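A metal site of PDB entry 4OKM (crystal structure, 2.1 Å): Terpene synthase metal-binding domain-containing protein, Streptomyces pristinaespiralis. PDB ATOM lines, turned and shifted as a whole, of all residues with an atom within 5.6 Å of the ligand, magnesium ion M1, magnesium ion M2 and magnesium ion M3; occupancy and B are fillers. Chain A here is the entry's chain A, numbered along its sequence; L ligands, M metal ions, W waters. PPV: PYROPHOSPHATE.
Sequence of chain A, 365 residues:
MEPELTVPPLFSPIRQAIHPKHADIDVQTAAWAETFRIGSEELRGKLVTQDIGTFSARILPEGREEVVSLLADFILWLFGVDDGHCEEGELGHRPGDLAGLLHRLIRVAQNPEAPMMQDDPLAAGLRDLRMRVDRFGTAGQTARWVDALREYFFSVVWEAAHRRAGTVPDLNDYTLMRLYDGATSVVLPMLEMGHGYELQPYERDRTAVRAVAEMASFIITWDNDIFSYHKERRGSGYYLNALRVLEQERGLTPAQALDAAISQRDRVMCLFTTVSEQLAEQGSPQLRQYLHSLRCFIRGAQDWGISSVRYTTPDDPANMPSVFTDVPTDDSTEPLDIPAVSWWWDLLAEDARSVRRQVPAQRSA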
ATOM      1  N   PHE A  79      -4.067 -10.918  28.131  1.00  0.00           N
ATOM      2  CA  PHE A  79      -4.003 -12.188  27.391  1.00  0.00           C
ATOM      3  C   PHE A  79      -5.223 -13.060  27.728  1.00  0.00           C
ATOM      4  O   PHE A  79      -5.728 -13.778  26.876  1.00  0.00           O
ATOM      5  CB  PHE A  79      -2.695 -12.933  27.656  1.00  0.00           C
ATOM      6  CG  PHE A  79      -1.502 -12.335  26.964  1.00  0.00           C
ATOM      7  CD1 PHE A  79      -0.375 -11.965  27.671  1.00  0.00           C
ATOM      8  CD2 PHE A  79      -1.512 -12.134  25.584  1.00  0.00           C
ATOM      9  CE1 PHE A  79       0.718 -11.416  27.025  1.00  0.00           C
ATOM     10  CE2 PHE A  79      -0.425 -11.589  24.931  1.00  0.00           C
ATOM     11  CZ  PHE A  79       0.686 -11.220  25.655  1.00  0.00           C
ATOM     12  N   ASP A  82      -7.552 -11.496  25.315  1.00  0.00           N
ATOM     13  CA  ASP A  82      -7.086 -11.584  23.922  1.00  0.00           C
ATOM     14  C   ASP A  82      -6.950 -13.042  23.429  1.00  0.00           C
ATOM     15  O   ASP A  82      -7.380 -13.364  22.312  1.00  0.00           O
ATOM     16  CB  ASP A  82      -5.767 -10.824  23.735  1.00  0.00           C
ATOM     17  CG  ASP A  82      -5.583 -10.335  22.301  1.00  0.00           C
ATOM     18  OD1 ASP A  82      -6.369  -9.482  21.855  1.00  0.00           O
ATOM     19  OD2 ASP A  82      -4.650 -10.811  21.624  1.00  0.00           O
ATOM     20  N   ASP A  83      -6.356 -13.902  24.236  1.00  0.00           N
ATOM     21  CA  ASP A  83      -6.298 -15.335  23.922  1.00  0.00           C
ATOM     22  C   ASP A  83      -7.652 -15.993  24.188  1.00  0.00           C
ATOM     23  O   ASP A  83      -8.235 -16.619  23.300  1.00  0.00           O
ATOM     24  CB  ASP A  83      -5.214 -16.049  24.733  1.00  0.00           C
ATOM     25  CG  ASP A  83      -3.807 -15.636  24.343  1.00  0.00           C
ATOM     26  OD1 ASP A  83      -2.861 -15.966  25.088  1.00  0.00           O
ATOM     27  OD2 ASP A  83      -3.636 -14.986  23.287  1.00  0.00           O
ATOM     28  N   GLU A  87      -8.776 -14.551  20.154  1.00  0.00           N
ATOM     29  CA  GLU A  87      -8.036 -15.406  19.203  1.00  0.00           C
ATOM     30  C   GLU A  87      -8.242 -16.922  19.359  1.00  0.00           C
ATOM     31  O   GLU A  87      -8.016 -17.667  18.400  1.00  0.00           O
ATOM     32  CB  GLU A  87      -6.548 -15.095  19.265  1.00  0.00           C
ATOM     33  CG  GLU A  87      -6.227 -13.639  18.959  1.00  0.00           C
ATOM     34  CD  GLU A  87      -4.758 -13.411  18.638  1.00  0.00           C
ATOM     35  OE1 GLU A  87      -4.274 -13.932  17.618  1.00  0.00           O
ATOM     36  OE2 GLU A  87      -4.080 -12.702  19.420  1.00  0.00           O
ATOM     37  N   VAL A 156     -10.129  -4.806  18.576  1.00  0.00           N
ATOM     38  CA  VAL A 156     -10.257  -6.267  18.480  1.00  0.00           C
ATOM     39  C   VAL A 156     -11.645  -6.717  17.999  1.00  0.00           C
ATOM     40  O   VAL A 156     -11.791  -7.837  17.511  1.00  0.00           O
ATOM     41  CB  VAL A 156      -9.837  -7.039  19.764  1.00  0.00           C
ATOM     42  CG1 VAL A 156      -8.331  -6.937  19.960  1.00  0.00           C
ATOM     43  CG2 VAL A 156     -10.608  -6.607  20.992  1.00  0.00           C
ATOM     44  N   GLU A 159     -10.854  -6.513  14.403  1.00  0.00           N
ATOM     45  CA  GLU A 159     -10.088  -7.715  14.080  1.00  0.00           C
ATOM     46  C   GLU A 159     -10.995  -8.952  13.996  1.00  0.00           C
ATOM     47  O   GLU A 159     -10.823  -9.810  13.128  1.00  0.00           O
ATOM     48  CB  GLU A 159      -8.985  -7.961  15.112  1.00  0.00           C
ATOM     49  CG  GLU A 159      -8.023  -9.073  14.742  1.00  0.00           C
ATOM     50  CD  GLU A 159      -7.175  -9.567  15.924  1.00  0.00           C
ATOM     51  OE1 GLU A 159      -7.736  -9.933  16.974  1.00  0.00           O
ATOM     52  OE2 GLU A 159      -5.949  -9.616  15.783  1.00  0.00           O
ATOM     53  N   ARG A 178      -3.683  -2.225  14.134  1.00  0.00           N
ATOM     54  CA  ARG A 178      -2.578  -2.775  14.912  1.00  0.00           C
ATOM     55  C   ARG A 178      -2.000  -1.769  15.904  1.00  0.00           C
ATOM     56  O   ARG A 178      -1.420  -2.138  16.912  1.00  0.00           O
ATOM     57  CB  ARG A 178      -1.482  -3.295  13.969  1.00  0.00           C
ATOM     58  CG  ARG A 178      -0.428  -4.180  14.609  1.00  0.00           C
ATOM     59  CD  ARG A 178      -1.023  -5.357  15.355  1.00  0.00           C
ATOM     60  NE  ARG A 178      -0.006  -6.340  15.731  1.00  0.00           N
ATOM     61  CZ  ARG A 178      -0.068  -7.121  16.808  1.00  0.00           C
ATOM     62  NH1 ARG A 178       0.926  -7.966  17.064  1.00  0.00           N
ATOM     63  NH2 ARG A 178      -1.105  -7.066  17.649  1.00  0.00           N
ATOM     64  N   ASP A 181      -4.804  -2.873  18.696  1.00  0.00           N
ATOM     65  CA  ASP A 181      -5.256  -4.244  19.009  1.00  0.00           C
ATOM     66  C   ASP A 181      -4.205  -5.119  19.677  1.00  0.00           C
ATOM     67  O   ASP A 181      -4.520  -6.226  20.103  1.00  0.00           O
ATOM     68  CB  ASP A 181      -5.905  -4.942  17.778  1.00  0.00           C
ATOM     69  CG  ASP A 181      -4.896  -5.524  16.795  1.00  0.00           C
ATOM     70  OD1 ASP A 181      -5.355  -5.937  15.705  1.00  0.00           O
ATOM     71  OD2 ASP A 181      -3.685  -5.598  17.066  1.00  0.00           O
ATOM     72  N   GLY A 182      -2.983  -4.615  19.771  1.00  0.00           N
ATOM     73  CA  GLY A 182      -1.927  -5.260  20.551  1.00  0.00           C
ATOM     74  C   GLY A 182      -1.940  -4.846  22.012  1.00  0.00           C
ATOM     75  O   GLY A 182      -1.085  -5.294  22.788  1.00  0.00           O
ATOM     76  N   ASN A 224       6.658  -7.811  17.466  1.00  0.00           N
ATOM     77  CA  ASN A 224       5.849  -8.963  17.834  1.00  0.00           C
ATOM     78  C   ASN A 224       5.397  -9.767  16.612  1.00  0.00           C
ATOM     79  O   ASN A 224       5.495 -10.993  16.614  1.00  0.00           O
ATOM     80  CB  ASN A 224       4.633  -8.561  18.667  1.00  0.00           C
ATOM     81  CG  ASN A 224       3.712  -9.730  18.929  1.00  0.00           C
ATOM     82  OD1 ASN A 224       2.857 -10.049  18.098  1.00  0.00           O
ATOM     83  ND2 ASN A 224       3.873 -10.383  20.066  1.00  0.00           N
ATOM     84  N   ASP A 225       4.914  -9.088  15.582  1.00  0.00           N
ATOM     85  CA  ASP A 225       4.549  -9.778  14.337  1.00  0.00           C
ATOM     86  C   ASP A 225       5.715 -10.634  13.830  1.00  0.00           C
ATOM     87  O   ASP A 225       5.498 -11.762  13.373  1.00  0.00           O
ATOM     88  CB  ASP A 225       4.107  -8.800  13.249  1.00  0.00           C
ATOM     89  CG  ASP A 225       2.724  -8.225  13.504  1.00  0.00           C
ATOM     90  OD1 ASP A 225       2.236  -7.471  12.631  1.00  0.00           O
ATOM     91  OD2 ASP A 225       2.117  -8.525  14.561  1.00  0.00           O
ATOM     92  N   SER A 228       6.515 -13.457  16.845  1.00  0.00           N
ATOM     93  CA  SER A 228       5.384 -14.371  17.076  1.00  0.00           C
ATOM     94  C   SER A 228       4.857 -15.016  15.789  1.00  0.00           C
ATOM     95  O   SER A 228       3.942 -15.836  15.848  1.00  0.00           O
ATOM     96  CB  SER A 228       4.244 -13.652  17.817  1.00  0.00           C
ATOM     97  OG  SER A 228       3.498 -12.764  16.989  1.00  0.00           O
ATOM     98  N   LYS A 231       4.994 -18.882  16.042  1.00  0.00           N
ATOM     99  CA  LYS A 231       3.931 -19.339  16.948  1.00  0.00           C
ATOM    100  C   LYS A 231       2.528 -19.207  16.314  1.00  0.00           C
ATOM    101  O   LYS A 231       1.668 -20.058  16.513  1.00  0.00           O
ATOM    102  CB  LYS A 231       4.028 -18.538  18.270  1.00  0.00           C
ATOM    103  CG  LYS A 231       2.845 -18.663  19.205  1.00  0.00           C
ATOM    104  CD  LYS A 231       1.732 -17.669  18.868  1.00  0.00           C
ATOM    105  CE  LYS A 231       1.722 -16.446  19.765  1.00  0.00           C
ATOM    106  NZ  LYS A 231       0.344 -15.881  19.820  1.00  0.00           N
ATOM    107  N   GLU A 232       2.317 -18.146  15.540  1.00  0.00           N
ATOM    108  CA  GLU A 232       1.020 -17.869  14.936  1.00  0.00           C
ATOM    109  C   GLU A 232       0.769 -18.684  13.670  1.00  0.00           C
ATOM    110  O   GLU A 232      -0.290 -19.311  13.533  1.00  0.00           O
ATOM    111  CB  GLU A 232       0.871 -16.370  14.639  1.00  0.00           C
ATOM    112  CG  GLU A 232       0.649 -15.555  15.904  1.00  0.00           C
ATOM    113  CD  GLU A 232       0.791 -14.055  15.694  1.00  0.00           C
ATOM    114  OE1 GLU A 232       0.762 -13.325  16.716  1.00  0.00           O
ATOM    115  OE2 GLU A 232       0.944 -13.606  14.533  1.00  0.00           O
ATOM    116  N   LEU A 240      -3.433 -13.039  12.104  1.00  0.00           N
ATOM    117  CA  LEU A 240      -3.106 -11.829  11.351  1.00  0.00           C
ATOM    118  C   LEU A 240      -1.779 -11.299  11.824  1.00  0.00           C
ATOM    119  O   LEU A 240      -1.507 -11.287  13.029  1.00  0.00           O
ATOM    120  CB  LEU A 240      -4.155 -10.739  11.576  1.00  0.00           C
ATOM    121  CG  LEU A 240      -5.020 -10.287  10.415  1.00  0.00           C
ATOM    122  CD1 LEU A 240      -5.832  -9.071  10.842  1.00  0.00           C
ATOM    123  CD2 LEU A 240      -4.190  -9.979   9.188  1.00  0.00           C
ATOM    124  N   TRP A 304      11.892  -9.733  25.763  1.00  0.00           N
ATOM    125  CA  TRP A 304      10.863 -10.718  26.140  1.00  0.00           C
ATOM    126  C   TRP A 304      10.382 -11.508  24.920  1.00  0.00           C
ATOM    127  O   TRP A 304      10.119 -12.702  25.012  1.00  0.00           O
ATOM    128  CB  TRP A 304       9.697 -10.007  26.813  1.00  0.00           C
ATOM    129  CG  TRP A 304       8.593 -10.899  27.304  1.00  0.00           C
ATOM    130  CD1 TRP A 304       8.652 -11.799  28.329  1.00  0.00           C
ATOM    131  CD2 TRP A 304       7.246 -10.942  26.803  1.00  0.00           C
ATOM    132  NE1 TRP A 304       7.426 -12.412  28.490  1.00  0.00           N
ATOM    133  CE2 TRP A 304       6.552 -11.901  27.574  1.00  0.00           C
ATOM    134  CE3 TRP A 304       6.566 -10.263  25.789  1.00  0.00           C
ATOM    135  CZ2 TRP A 304       5.213 -12.202  27.351  1.00  0.00           C
ATOM    136  CZ3 TRP A 304       5.228 -10.563  25.580  1.00  0.00           C
ATOM    137  CH2 TRP A 304       4.564 -11.522  26.354  1.00  0.00           C
ATOM    138  N   ARG A 310       6.179 -18.265  25.201  1.00  0.00           N
ATOM    139  CA  ARG A 310       5.061 -17.845  24.367  1.00  0.00           C
ATOM    140  C   ARG A 310       5.476 -17.752  22.897  1.00  0.00           C
ATOM    141  O   ARG A 310       4.691 -18.037  21.997  1.00  0.00           O
ATOM    142  CB  ARG A 310       4.516 -16.491  24.834  1.00  0.00           C
ATOM    143  CG  ARG A 310       3.254 -16.051  24.115  1.00  0.00           C
ATOM    144  CD  ARG A 310       2.718 -14.728  24.635  1.00  0.00           C
ATOM    145  NE  ARG A 310       1.509 -14.387  23.899  1.00  0.00           N
ATOM    146  CZ  ARG A 310       0.269 -14.801  24.183  1.00  0.00           C
ATOM    147  NH1 ARG A 310      -0.732 -14.426  23.404  1.00  0.00           N
ATOM    148  NH2 ARG A 310       0.022 -15.583  25.233  1.00  0.00           N
ATOM    149  N   TYR A 311       6.735 -17.349  22.654  1.00  0.00           N
ATOM    150  CA  TYR A 311       7.237 -17.180  21.281  1.00  0.00           C
ATOM    151  C   TYR A 311       8.288 -18.228  20.878  1.00  0.00           C
ATOM    152  O   TYR A 311       8.369 -18.597  19.698  1.00  0.00           O
ATOM    153  CB  TYR A 311       7.770 -15.751  21.103  1.00  0.00           C
ATOM    154  CG  TYR A 311       6.785 -14.699  21.568  1.00  0.00           C
ATOM    155  CD1 TYR A 311       7.082 -13.870  22.656  1.00  0.00           C
ATOM    156  CD2 TYR A 311       5.545 -14.571  20.973  1.00  0.00           C
ATOM    157  CE1 TYR A 311       6.168 -12.928  23.095  1.00  0.00           C
ATOM    158  CE2 TYR A 311       4.618 -13.627  21.407  1.00  0.00           C
ATOM    159  CZ  TYR A 311       4.931 -12.811  22.472  1.00  0.00           C
ATOM    160  OH  TYR A 311       4.026 -11.888  22.920  1.00  0.00           O
HETATM  161  O11 PPV L   1       1.629 -12.393  22.057  1.00  0.00           O
HETATM  162  P1  PPV L   1       0.869 -12.379  20.757  1.00  0.00           P
HETATM  163  O21 PPV L   1       1.733 -12.465  19.510  1.00  0.00           O
HETATM  164  O31 PPV L   1      -0.302 -13.316  20.745  1.00  0.00           O
HETATM  165  OPP PPV L   1       0.229 -10.895  20.728  1.00  0.00           O
HETATM  166  P2  PPV L   1      -0.734 -10.382  19.529  1.00  0.00           P
HETATM  167  O12 PPV L   1      -0.890  -8.915  19.830  1.00  0.00           O
HETATM  168  O22 PPV L   1      -2.000 -11.189  19.686  1.00  0.00           O
HETATM  169  O32 PPV L   1       0.010 -10.665  18.245  1.00  0.00           O
HETATM  170 MG    MG M   1       1.575 -11.691  17.629  1.00  0.00          MG
HETATM  171 MG    MG M   2      -2.167 -13.173  20.222  1.00  0.00          MG
HETATM  172 MG    MG M   3      -4.179 -10.564  19.566  1.00  0.00          MG
HETATM  173  O   HOH W   1      -1.615 -13.849  18.301  1.00  0.00           O
HETATM  174  O   HOH W   2      -6.248 -10.347  19.225  1.00  0.00           O
HETATM  175  O   HOH W   3      -2.714 -15.169  20.741  1.00  0.00           O
HETATM  176  O   HOH W   4       1.607 -10.938  15.570  1.00  0.00           O
HETATM  177  O   HOH W   5      -3.926 -10.493  17.502  1.00  0.00           O
HETATM  178  O   HOH W   6      -3.573  -8.727  20.016  1.00  0.00           O
HETATM  179  O   HOH W   7      -2.752 -12.606  22.159  1.00  0.00           O
HETATM  180  O   HOH W   8      -1.690 -11.163  16.138  1.00  0.00           O
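NH2 of Arg 178 is in salt-bridge range of O12 of the ligand (2.9 Å).
The guanidinium group of Arg 310 is in salt-bridge range of an oxygen (O11) of the ligand.
The side-chain amino group of Lys 231 sits close to an oxygen (O31) of the ligand, 2.8 Å away.
An oxygen (O11) of the ligand is in hydrogen-bond range of the side-chain hydroxyl (OH) of Tyr 311, 2.6 Å away.
The guanidinium group (NH2) of Arg 178 is in salt-bridge range of the side-chain carboxylate (OD2) of Asp 181, at 3.0 Å.
The guanidinium group of Arg 310 lies within salt-bridge range of the side-chain carboxylate of Asp 83, 2.9 Å away.
OD2 of Asp 225 lies within salt-bridge range of NH1 of Arg 178 (2.8 Å).
OD1 of Asn 224 lies close to NH1 of Arg 178 (3.0 Å).
OH of Tyr 311 is in hydrogen-bond range of ND2 of Asn 224.
Merely in contact with the ligand: Phe 79 and Gly 182.
Of the 18 residues printed, 11 come within 4 Å of the ligand.
The nearest printed residue that does not touch the ligand is Asp 83 (4.5 Å).
Arg 178 touches magnesium ion M1.
Within 4 Å of magnesium ion M1: Arg 178, Asn 224, Ser 228 and Glu 232.
Merely in contact with magnesium ion M2: Asp 83 (3.9 Å), Lys 231 (3.7 Å) and Arg 310 (3.7 Å).
The nearest printed residue that does not touch magnesium ion M2 is Glu 232 (4.6 Å).
The nearest printed residue that does not touch magnesium ion M3 is Glu 159 (4.3 Å).
Magnesium ion M1 is bound by an oxygen (O32) of the ligand (2.0 Å).
Magnesium ion M1 is bound by OE1 of Glu 232, at 2.0 Å.
An oxygen (O21) of the ligand binds magnesium ion M1 (2.0 Å).
Magnesium ion M1 is bound by OD1 of Asn 224.
Magnesium ion M1 is bound by water W4, at 2.2 Å.
Magnesium ion M1 is bound by OG of Ser 228, 2.3 Å away.
Magnesium ion M1 has six donor atoms within binding distance.
Magnesium ion M2 is bound by O31 of the ligand (1.9 Å), O22 of the ligand (2.1 Å), water W7 (2.1 Å), water W1 (2.1 Å), OE2 of Glu 87 (2.1 Å) and water W3 (2.1 Å).
Magnesium ion M3 is bound by water W6 (2.0 Å), water W5 (2.1 Å), water W2 (2.1 Å), the side-chain carboxylate of Asp 82 (2.1 Å), the side-chain carboxylate of Glu 87 (2.1 Å) and an oxygen (O22) of the ligand (2.3 Å).
Water W4 lies within hydrogen-bond range of OD2 of Asp 225, OE2 of Glu 232 and NH1 of Arg 178.
Water W7 bridges OD2 of Asp 83 (2.8 Å) and NH1 of Arg 310 (3.0 Å).
Water W1 bridges the side-chain carboxylate (OE1) of Glu 87 (2.7 Å) and the side-chain amino group (NZ) of Lys 231 (3.2 Å).
Water W3 lies within hydrogen-bond range of the side-chain carboxylate of Asp 83 (2.7 Å), the side-chain amino group of Lys 231 (3.3 Å) and the guanidinium group of Arg 310 (3.4 Å).
Water W2 bridges OE1 of Glu 159 (2.7 Å) and OD1 of Asp 82 (2.8 Å).
Water W6 lies within hydrogen-bond range of the backbone carbonyl oxygen of Asp 181 (2.7 Å), an oxygen (O12) of the ligand (2.7 Å) and the side-chain carboxylate of Asp 82 (3.4 Å).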
